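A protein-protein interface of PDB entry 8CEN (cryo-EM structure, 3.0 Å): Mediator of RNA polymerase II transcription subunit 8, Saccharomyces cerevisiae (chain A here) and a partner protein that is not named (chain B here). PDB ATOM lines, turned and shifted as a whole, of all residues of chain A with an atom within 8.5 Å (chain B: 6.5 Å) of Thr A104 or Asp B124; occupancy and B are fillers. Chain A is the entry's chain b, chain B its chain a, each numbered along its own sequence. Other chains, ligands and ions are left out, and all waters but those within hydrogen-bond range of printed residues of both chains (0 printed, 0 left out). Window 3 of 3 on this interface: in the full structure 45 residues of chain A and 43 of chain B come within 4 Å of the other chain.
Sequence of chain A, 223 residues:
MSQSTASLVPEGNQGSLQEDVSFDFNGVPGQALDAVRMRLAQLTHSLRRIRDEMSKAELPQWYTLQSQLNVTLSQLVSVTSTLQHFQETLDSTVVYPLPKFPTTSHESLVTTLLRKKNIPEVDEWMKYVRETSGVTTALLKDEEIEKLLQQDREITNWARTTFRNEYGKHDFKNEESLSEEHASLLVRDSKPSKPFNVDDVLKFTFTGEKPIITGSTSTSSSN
The backbone carbonyl oxygen of Pro A99 is in hydrogen-bond range of the guanidinium group of Arg B121 (3.1 Å). The guanidinium group of Arg B121 is in hydrogen-bond range of the backbone carbonyl oxygen of Phe A101, 3.4 Å away. The side-chain hydroxyl of Thr A103 is in hydrogen-bond range of the guanidinium group of Arg B121, at 2.9 Å. OG1 of Thr A104 is in hydrogen-bond range of OD1 of Asp B124, at 2.9 Å.
Among the printed residues, merely in contact across the chains: Pro A99 with Phe B125, Thr A103 with Asp B124, Thr A103 with Phe B125, Thr A103 with Ile B156, Thr A104 with Arg B121, Glu A107 with Ile B156 and Val A110 with Ile B156.
Printed residues of chain B within 4 Å of Pro A99: Arg B121 (3.1 Å) and Phe B125 (3.5 Å). Printed residues of chain B within 4 Å of Phe A101: Arg B121 (3.4 Å). Thr A104 touches just these residues of chain B: Arg B121 and Asp B124. Printed residues of chain B within 4 Å of Glu A107: Ile B156 (3.5 Å). No residue of chain A comes within 4 Å of Pro B123. Asp B124 touches just these residues of chain A: Thr A103 and Thr A104. The nearest printed residue of chain A that does not touch Ile B156 is Thr A104 (4.6 Å).
Of the 10 printed residues of chain B, 4 touch a printed residue of chain A. Hydrophobic or aromatic side chains of chain B within 4 Å of the printed part of chain A: Phe B125 and Ile B156. Of the 11 printed residues of chain A, 6 touch a printed residue of chain B. Among the printed residues, 11 pairs touch across the chains. Among the printed residues, no Asp or Glu carboxylate lies within 4 Å of a Lys or Arg side-chain nitrogen of the other chain.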
ATOM      1  N   PRO A  99       3.731 -11.244 -34.072  1.00  0.00           N
ATOM      2  CA  PRO A  99       2.851 -10.100 -34.367  1.00  0.00           C
ATOM      3  C   PRO A  99       1.534 -10.480 -35.025  1.00  0.00           C
ATOM      4  O   PRO A  99       0.509  -9.859 -34.726  1.00  0.00           O
ATOM      5  CB  PRO A  99       3.715  -9.230 -35.286  1.00  0.00           C
ATOM      6  CG  PRO A  99       5.096  -9.502 -34.832  1.00  0.00           C
ATOM      7  CD  PRO A  99       5.127 -10.956 -34.459  1.00  0.00           C
ATOM      8  N   PHE A 101      -0.359 -12.882 -34.396  1.00  0.00           N
ATOM      9  CA  PHE A 101      -1.331 -13.176 -33.346  1.00  0.00           C
ATOM     10  C   PHE A 101      -2.074 -11.897 -32.973  1.00  0.00           C
ATOM     11  O   PHE A 101      -1.438 -10.860 -32.750  1.00  0.00           O
ATOM     12  CB  PHE A 101      -0.637 -13.751 -32.105  1.00  0.00           C
ATOM     13  CG  PHE A 101      -1.549 -14.546 -31.195  1.00  0.00           C
ATOM     14  CD1 PHE A 101      -2.500 -13.914 -30.407  1.00  0.00           C
ATOM     15  CD2 PHE A 101      -1.432 -15.920 -31.106  1.00  0.00           C
ATOM     16  CE1 PHE A 101      -3.329 -14.636 -29.582  1.00  0.00           C
ATOM     17  CE2 PHE A 101      -2.256 -16.650 -30.274  1.00  0.00           C
ATOM     18  CZ  PHE A 101      -3.202 -16.006 -29.506  1.00  0.00           C
ATOM     19  N   PRO A 102      -3.403 -11.925 -32.887  1.00  0.00           N
ATOM     20  CA  PRO A 102      -4.119 -10.774 -32.322  1.00  0.00           C
ATOM     21  C   PRO A 102      -3.932 -10.692 -30.816  1.00  0.00           C
ATOM     22  O   PRO A 102      -4.553 -11.444 -30.060  1.00  0.00           O
ATOM     23  CB  PRO A 102      -5.580 -11.046 -32.699  1.00  0.00           C
ATOM     24  CG  PRO A 102      -5.654 -12.520 -32.920  1.00  0.00           C
ATOM     25  CD  PRO A 102      -4.315 -12.937 -33.445  1.00  0.00           C
ATOM     26  N   THR A 103      -3.091  -9.762 -30.367  1.00  0.00           N
ATOM     27  CA  THR A 103      -2.741  -9.659 -28.957  1.00  0.00           C
ATOM     28  C   THR A 103      -3.570  -8.632 -28.204  1.00  0.00           C
ATOM     29  O   THR A 103      -3.849  -8.832 -27.018  1.00  0.00           O
ATOM     30  CB  THR A 103      -1.258  -9.309 -28.802  1.00  0.00           C
ATOM     31  OG1 THR A 103      -0.973  -8.102 -29.518  1.00  0.00           O
ATOM     32  CG2 THR A 103      -0.391 -10.433 -29.347  1.00  0.00           C
ATOM     33  N   THR A 104      -3.957  -7.535 -28.856  1.00  0.00           N
ATOM     34  CA  THR A 104      -4.813  -6.551 -28.202  1.00  0.00           C
ATOM     35  C   THR A 104      -6.216  -7.105 -27.982  1.00  0.00           C
ATOM     36  O   THR A 104      -6.798  -6.931 -26.904  1.00  0.00           O
ATOM     37  CB  THR A 104      -4.864  -5.268 -29.031  1.00  0.00           C
ATOM     38  OG1 THR A 104      -3.530  -4.805 -29.278  1.00  0.00           O
ATOM     39  CG2 THR A 104      -5.641  -4.185 -28.300  1.00  0.00           C
ATOM     40  N   SER A 105      -6.766  -7.789 -28.984  1.00  0.00           N
ATOM     41  CA  SER A 105      -8.136  -8.272 -28.901  1.00  0.00           C
ATOM     42  C   SER A 105      -8.269  -9.566 -28.111  1.00  0.00           C
ATOM     43  O   SER A 105      -9.360  -9.856 -27.611  1.00  0.00           O
ATOM     44  CB  SER A 105      -8.708  -8.476 -30.305  1.00  0.00           C
ATOM     45  OG  SER A 105      -8.150  -9.624 -30.918  1.00  0.00           O
ATOM     46  N   HIS A 106      -7.202 -10.351 -27.992  1.00  0.00           N
ATOM     47  CA  HIS A 106      -7.268 -11.651 -27.330  1.00  0.00           C
ATOM     48  C   HIS A 106      -6.058 -11.848 -26.419  1.00  0.00           C
ATOM     49  O   HIS A 106      -5.396 -12.888 -26.434  1.00  0.00           O
ATOM     50  CB  HIS A 106      -7.402 -12.769 -28.362  1.00  0.00           C
ATOM     51  CG  HIS A 106      -8.713 -12.757 -29.083  1.00  0.00           C
ATOM     52  ND1 HIS A 106      -8.909 -12.068 -30.260  1.00  0.00           N
ATOM     53  CD2 HIS A 106      -9.901 -13.329 -28.781  1.00  0.00           C
ATOM     54  CE1 HIS A 106     -10.159 -12.226 -30.659  1.00  0.00           C
ATOM     55  NE2 HIS A 106     -10.781 -12.989 -29.779  1.00  0.00           N
ATOM     56  N   GLU A 107      -5.766 -10.820 -25.614  1.00  0.00           N
ATOM     57  CA  GLU A 107      -4.733 -10.938 -24.589  1.00  0.00           C
ATOM     58  C   GLU A 107      -5.083 -12.021 -23.579  1.00  0.00           C
ATOM     59  O   GLU A 107      -4.211 -12.788 -23.154  1.00  0.00           O
ATOM     60  CB  GLU A 107      -4.532  -9.599 -23.880  1.00  0.00           C
ATOM     61  CG  GLU A 107      -3.415  -9.614 -22.846  1.00  0.00           C
ATOM     62  CD  GLU A 107      -3.201  -8.264 -22.191  1.00  0.00           C
ATOM     63  OE1 GLU A 107      -3.938  -7.315 -22.527  1.00  0.00           O
ATOM     64  OE2 GLU A 107      -2.295  -8.153 -21.339  1.00  0.00           O
ATOM     65  N   SER A 108      -6.358 -12.102 -23.192  1.00  0.00           N
ATOM     66  CA  SER A 108      -6.799 -13.160 -22.290  1.00  0.00           C
ATOM     67  C   SER A 108      -6.586 -14.534 -22.911  1.00  0.00           C
ATOM     68  O   SER A 108      -6.147 -15.466 -22.230  1.00  0.00           O
ATOM     69  CB  SER A 108      -8.268 -12.957 -21.923  1.00  0.00           C
ATOM     70  OG  SER A 108      -9.088 -12.992 -23.078  1.00  0.00           O
ATOM     71  N   LEU A 109      -6.862 -14.666 -24.211  1.00  0.00           N
ATOM     72  CA  LEU A 109      -6.696 -15.950 -24.886  1.00  0.00           C
ATOM     73  C   LEU A 109      -5.226 -16.352 -24.956  1.00  0.00           C
ATOM     74  O   LEU A 109      -4.880 -17.507 -24.675  1.00  0.00           O
ATOM     75  CB  LEU A 109      -7.326 -15.888 -26.282  1.00  0.00           C
ATOM     76  CG  LEU A 109      -7.480 -17.142 -27.153  1.00  0.00           C
ATOM     77  CD1 LEU A 109      -8.688 -16.976 -28.051  1.00  0.00           C
ATOM     78  CD2 LEU A 109      -6.257 -17.417 -28.019  1.00  0.00           C
ATOM     79  N   VAL A 110      -4.341 -15.416 -25.317  1.00  0.00           N
ATOM     80  CA  VAL A 110      -2.929 -15.774 -25.440  1.00  0.00           C
ATOM     81  C   VAL A 110      -2.318 -16.055 -24.067  1.00  0.00           C
ATOM     82  O   VAL A 110      -1.500 -16.970 -23.919  1.00  0.00           O
ATOM     83  CB  VAL A 110      -2.142 -14.707 -26.235  1.00  0.00           C
ATOM     84  CG1 VAL A 110      -2.130 -13.354 -25.553  1.00  0.00           C
ATOM     85  CG2 VAL A 110      -0.721 -15.180 -26.520  1.00  0.00           C
ATOM     86  N   ARG B 121       4.700  -5.202 -33.301  1.00  0.00           N
ATOM     87  CA  ARG B 121       3.483  -4.782 -33.985  1.00  0.00           C
ATOM     88  C   ARG B 121       3.046  -3.439 -33.427  1.00  0.00           C
ATOM     89  O   ARG B 121       2.761  -3.321 -32.228  1.00  0.00           O
ATOM     90  CB  ARG B 121       2.345  -5.792 -33.850  1.00  0.00           C
ATOM     91  CG  ARG B 121       1.378  -5.697 -35.024  1.00  0.00           C
ATOM     92  CD  ARG B 121       0.267  -6.719 -34.976  1.00  0.00           C
ATOM     93  NE  ARG B 121      -0.742  -6.416 -33.968  1.00  0.00           N
ATOM     94  CZ  ARG B 121      -0.799  -6.978 -32.768  1.00  0.00           C
ATOM     95  NH1 ARG B 121       0.092  -7.877 -32.383  1.00  0.00           N
ATOM     96  NH2 ARG B 121      -1.778  -6.635 -31.936  1.00  0.00           N
ATOM     97  N   GLU B 122       2.998  -2.437 -34.295  1.00  0.00           N
ATOM     98  CA  GLU B 122       2.468  -1.143 -33.913  1.00  0.00           C
ATOM     99  C   GLU B 122       0.952  -1.232 -33.741  1.00  0.00           C
ATOM    100  O   GLU B 122       0.289  -1.988 -34.458  1.00  0.00           O
ATOM    101  CB  GLU B 122       2.823  -0.094 -34.974  1.00  0.00           C
ATOM    102  CG  GLU B 122       4.325   0.146 -35.183  1.00  0.00           C
ATOM    103  CD  GLU B 122       5.013   0.945 -34.073  1.00  0.00           C
ATOM    104  OE1 GLU B 122       4.454   1.112 -32.968  1.00  0.00           O
ATOM    105  OE2 GLU B 122       6.146   1.409 -34.312  1.00  0.00           O
ATOM    106  N   PRO B 123       0.370  -0.483 -32.792  1.00  0.00           N
ATOM    107  CA  PRO B 123       1.073   0.364 -31.825  1.00  0.00           C
ATOM    108  C   PRO B 123       1.478  -0.374 -30.558  1.00  0.00           C
ATOM    109  O   PRO B 123       2.279   0.149 -29.789  1.00  0.00           O
ATOM    110  CB  PRO B 123       0.040   1.441 -31.506  1.00  0.00           C
ATOM    111  CG  PRO B 123      -1.255   0.717 -31.607  1.00  0.00           C
ATOM    112  CD  PRO B 123      -1.089  -0.288 -32.723  1.00  0.00           C
ATOM    113  N   ASP B 124       0.913  -1.573 -30.334  1.00  0.00           N
ATOM    114  CA  ASP B 124       1.046  -2.257 -29.048  1.00  0.00           C
ATOM    115  C   ASP B 124       1.248  -3.783 -29.153  1.00  0.00           C
ATOM    116  O   ASP B 124       0.349  -4.582 -28.880  1.00  0.00           O
ATOM    117  CB  ASP B 124      -0.166  -1.871 -28.189  1.00  0.00           C
ATOM    118  CG  ASP B 124      -1.509  -2.299 -28.808  1.00  0.00           C
ATOM    119  OD1 ASP B 124      -1.530  -2.859 -29.926  1.00  0.00           O
ATOM    120  OD2 ASP B 124      -2.556  -2.050 -28.182  1.00  0.00           O
ATOM    121  N   PHE B 125       2.495  -4.181 -29.439  1.00  0.00           N
ATOM    122  CA  PHE B 125       2.998  -5.532 -29.192  1.00  0.00           C
ATOM    123  C   PHE B 125       4.506  -5.548 -29.399  1.00  0.00           C
ATOM    124  O   PHE B 125       4.984  -5.072 -30.432  1.00  0.00           O
ATOM    125  CB  PHE B 125       2.352  -6.575 -30.111  1.00  0.00           C
ATOM    126  CG  PHE B 125       2.968  -7.932 -29.997  1.00  0.00           C
ATOM    127  CD1 PHE B 125       2.803  -8.678 -28.844  1.00  0.00           C
ATOM    128  CD2 PHE B 125       3.715  -8.462 -31.034  1.00  0.00           C
ATOM    129  CE1 PHE B 125       3.370  -9.927 -28.724  1.00  0.00           C
ATOM    130  CE2 PHE B 125       4.285  -9.713 -30.922  1.00  0.00           C
ATOM    131  CZ  PHE B 125       4.110 -10.446 -29.765  1.00  0.00           C
ATOM    132  N   TRP B 126       5.267  -6.098 -28.454  1.00  0.00           N
ATOM    133  CA  TRP B 126       6.715  -6.173 -28.611  1.00  0.00           C
ATOM    134  C   TRP B 126       7.222  -7.522 -28.118  1.00  0.00           C
ATOM    135  O   TRP B 126       6.549  -8.214 -27.358  1.00  0.00           O
ATOM    136  CB  TRP B 126       7.424  -5.038 -27.861  1.00  0.00           C
ATOM    137  CG  TRP B 126       7.033  -3.674 -28.327  1.00  0.00           C
ATOM    138  CD1 TRP B 126       7.644  -2.931 -29.288  1.00  0.00           C
ATOM    139  CD2 TRP B 126       5.940  -2.885 -27.845  1.00  0.00           C
ATOM    140  NE1 TRP B 126       7.000  -1.730 -29.442  1.00  0.00           N
ATOM    141  CE2 TRP B 126       5.948  -1.678 -28.567  1.00  0.00           C
ATOM    142  CE3 TRP B 126       4.954  -3.083 -26.874  1.00  0.00           C
ATOM    143  CZ2 TRP B 126       5.015  -0.671 -28.345  1.00  0.00           C
ATOM    144  CZ3 TRP B 126       4.027  -2.085 -26.659  1.00  0.00           C
ATOM    145  CH2 TRP B 126       4.065  -0.894 -27.389  1.00  0.00           C
ATOM    146  N   ILE B 155       5.431  -8.186 -24.775  1.00  0.00           N
ATOM    147  CA  ILE B 155       4.831  -6.970 -24.249  1.00  0.00           C
ATOM    148  C   ILE B 155       3.499  -6.812 -24.964  1.00  0.00           C
ATOM    149  O   ILE B 155       3.471  -6.608 -26.186  1.00  0.00           O
ATOM    150  CB  ILE B 155       5.712  -5.737 -24.512  1.00  0.00           C
ATOM    151  CG1 ILE B 155       7.208  -6.041 -24.351  1.00  0.00           C
ATOM    152  CG2 ILE B 155       5.313  -4.601 -23.583  1.00  0.00           C
ATOM    153  CD1 ILE B 155       7.650  -6.504 -23.014  1.00  0.00           C
ATOM    154  N   ILE B 156       2.403  -6.907 -24.220  1.00  0.00           N
ATOM    155  CA  ILE B 156       1.064  -6.761 -24.778  1.00  0.00           C
ATOM    156  C   ILE B 156       0.368  -5.674 -23.971  1.00  0.00           C
ATOM    157  O   ILE B 156      -0.037  -5.903 -22.824  1.00  0.00           O
ATOM    158  CB  ILE B 156       0.272  -8.072 -24.754  1.00  0.00           C
ATOM    159  CG1 ILE B 156       0.915  -9.102 -25.681  1.00  0.00           C
ATOM    160  CG2 ILE B 156      -1.160  -7.834 -25.199  1.00  0.00           C
ATOM    161  CD1 ILE B 156       0.397 -10.505 -25.474  1.00  0.00           C
ATOM    162  N   GLY B 157       0.228  -4.491 -24.565  1.00  0.00           N
ATOM    163  CA  GLY B 157      -0.426  -3.377 -23.908  1.00  0.00           C
ATOM    164  C   GLY B 157       0.297  -2.898 -22.669  1.00  0.00           C
ATOM    165  O   GLY B 157      -0.317  -2.751 -21.608  1.00  0.00           O
ATOM    166  N   ALA B 158       1.614  -2.716 -22.787  1.00  0.00           N
ATOM    167  CA  ALA B 158       2.499  -2.279 -21.707  1.00  0.00           C
ATOM    168  C   ALA B 158       2.481  -3.223 -20.508  1.00  0.00           C
ATOM    169  O   ALA B 158       2.851  -2.828 -19.401  1.00  0.00           O
ATOM    170  CB  ALA B 158       2.179  -0.850 -21.255  1.00  0.00           C
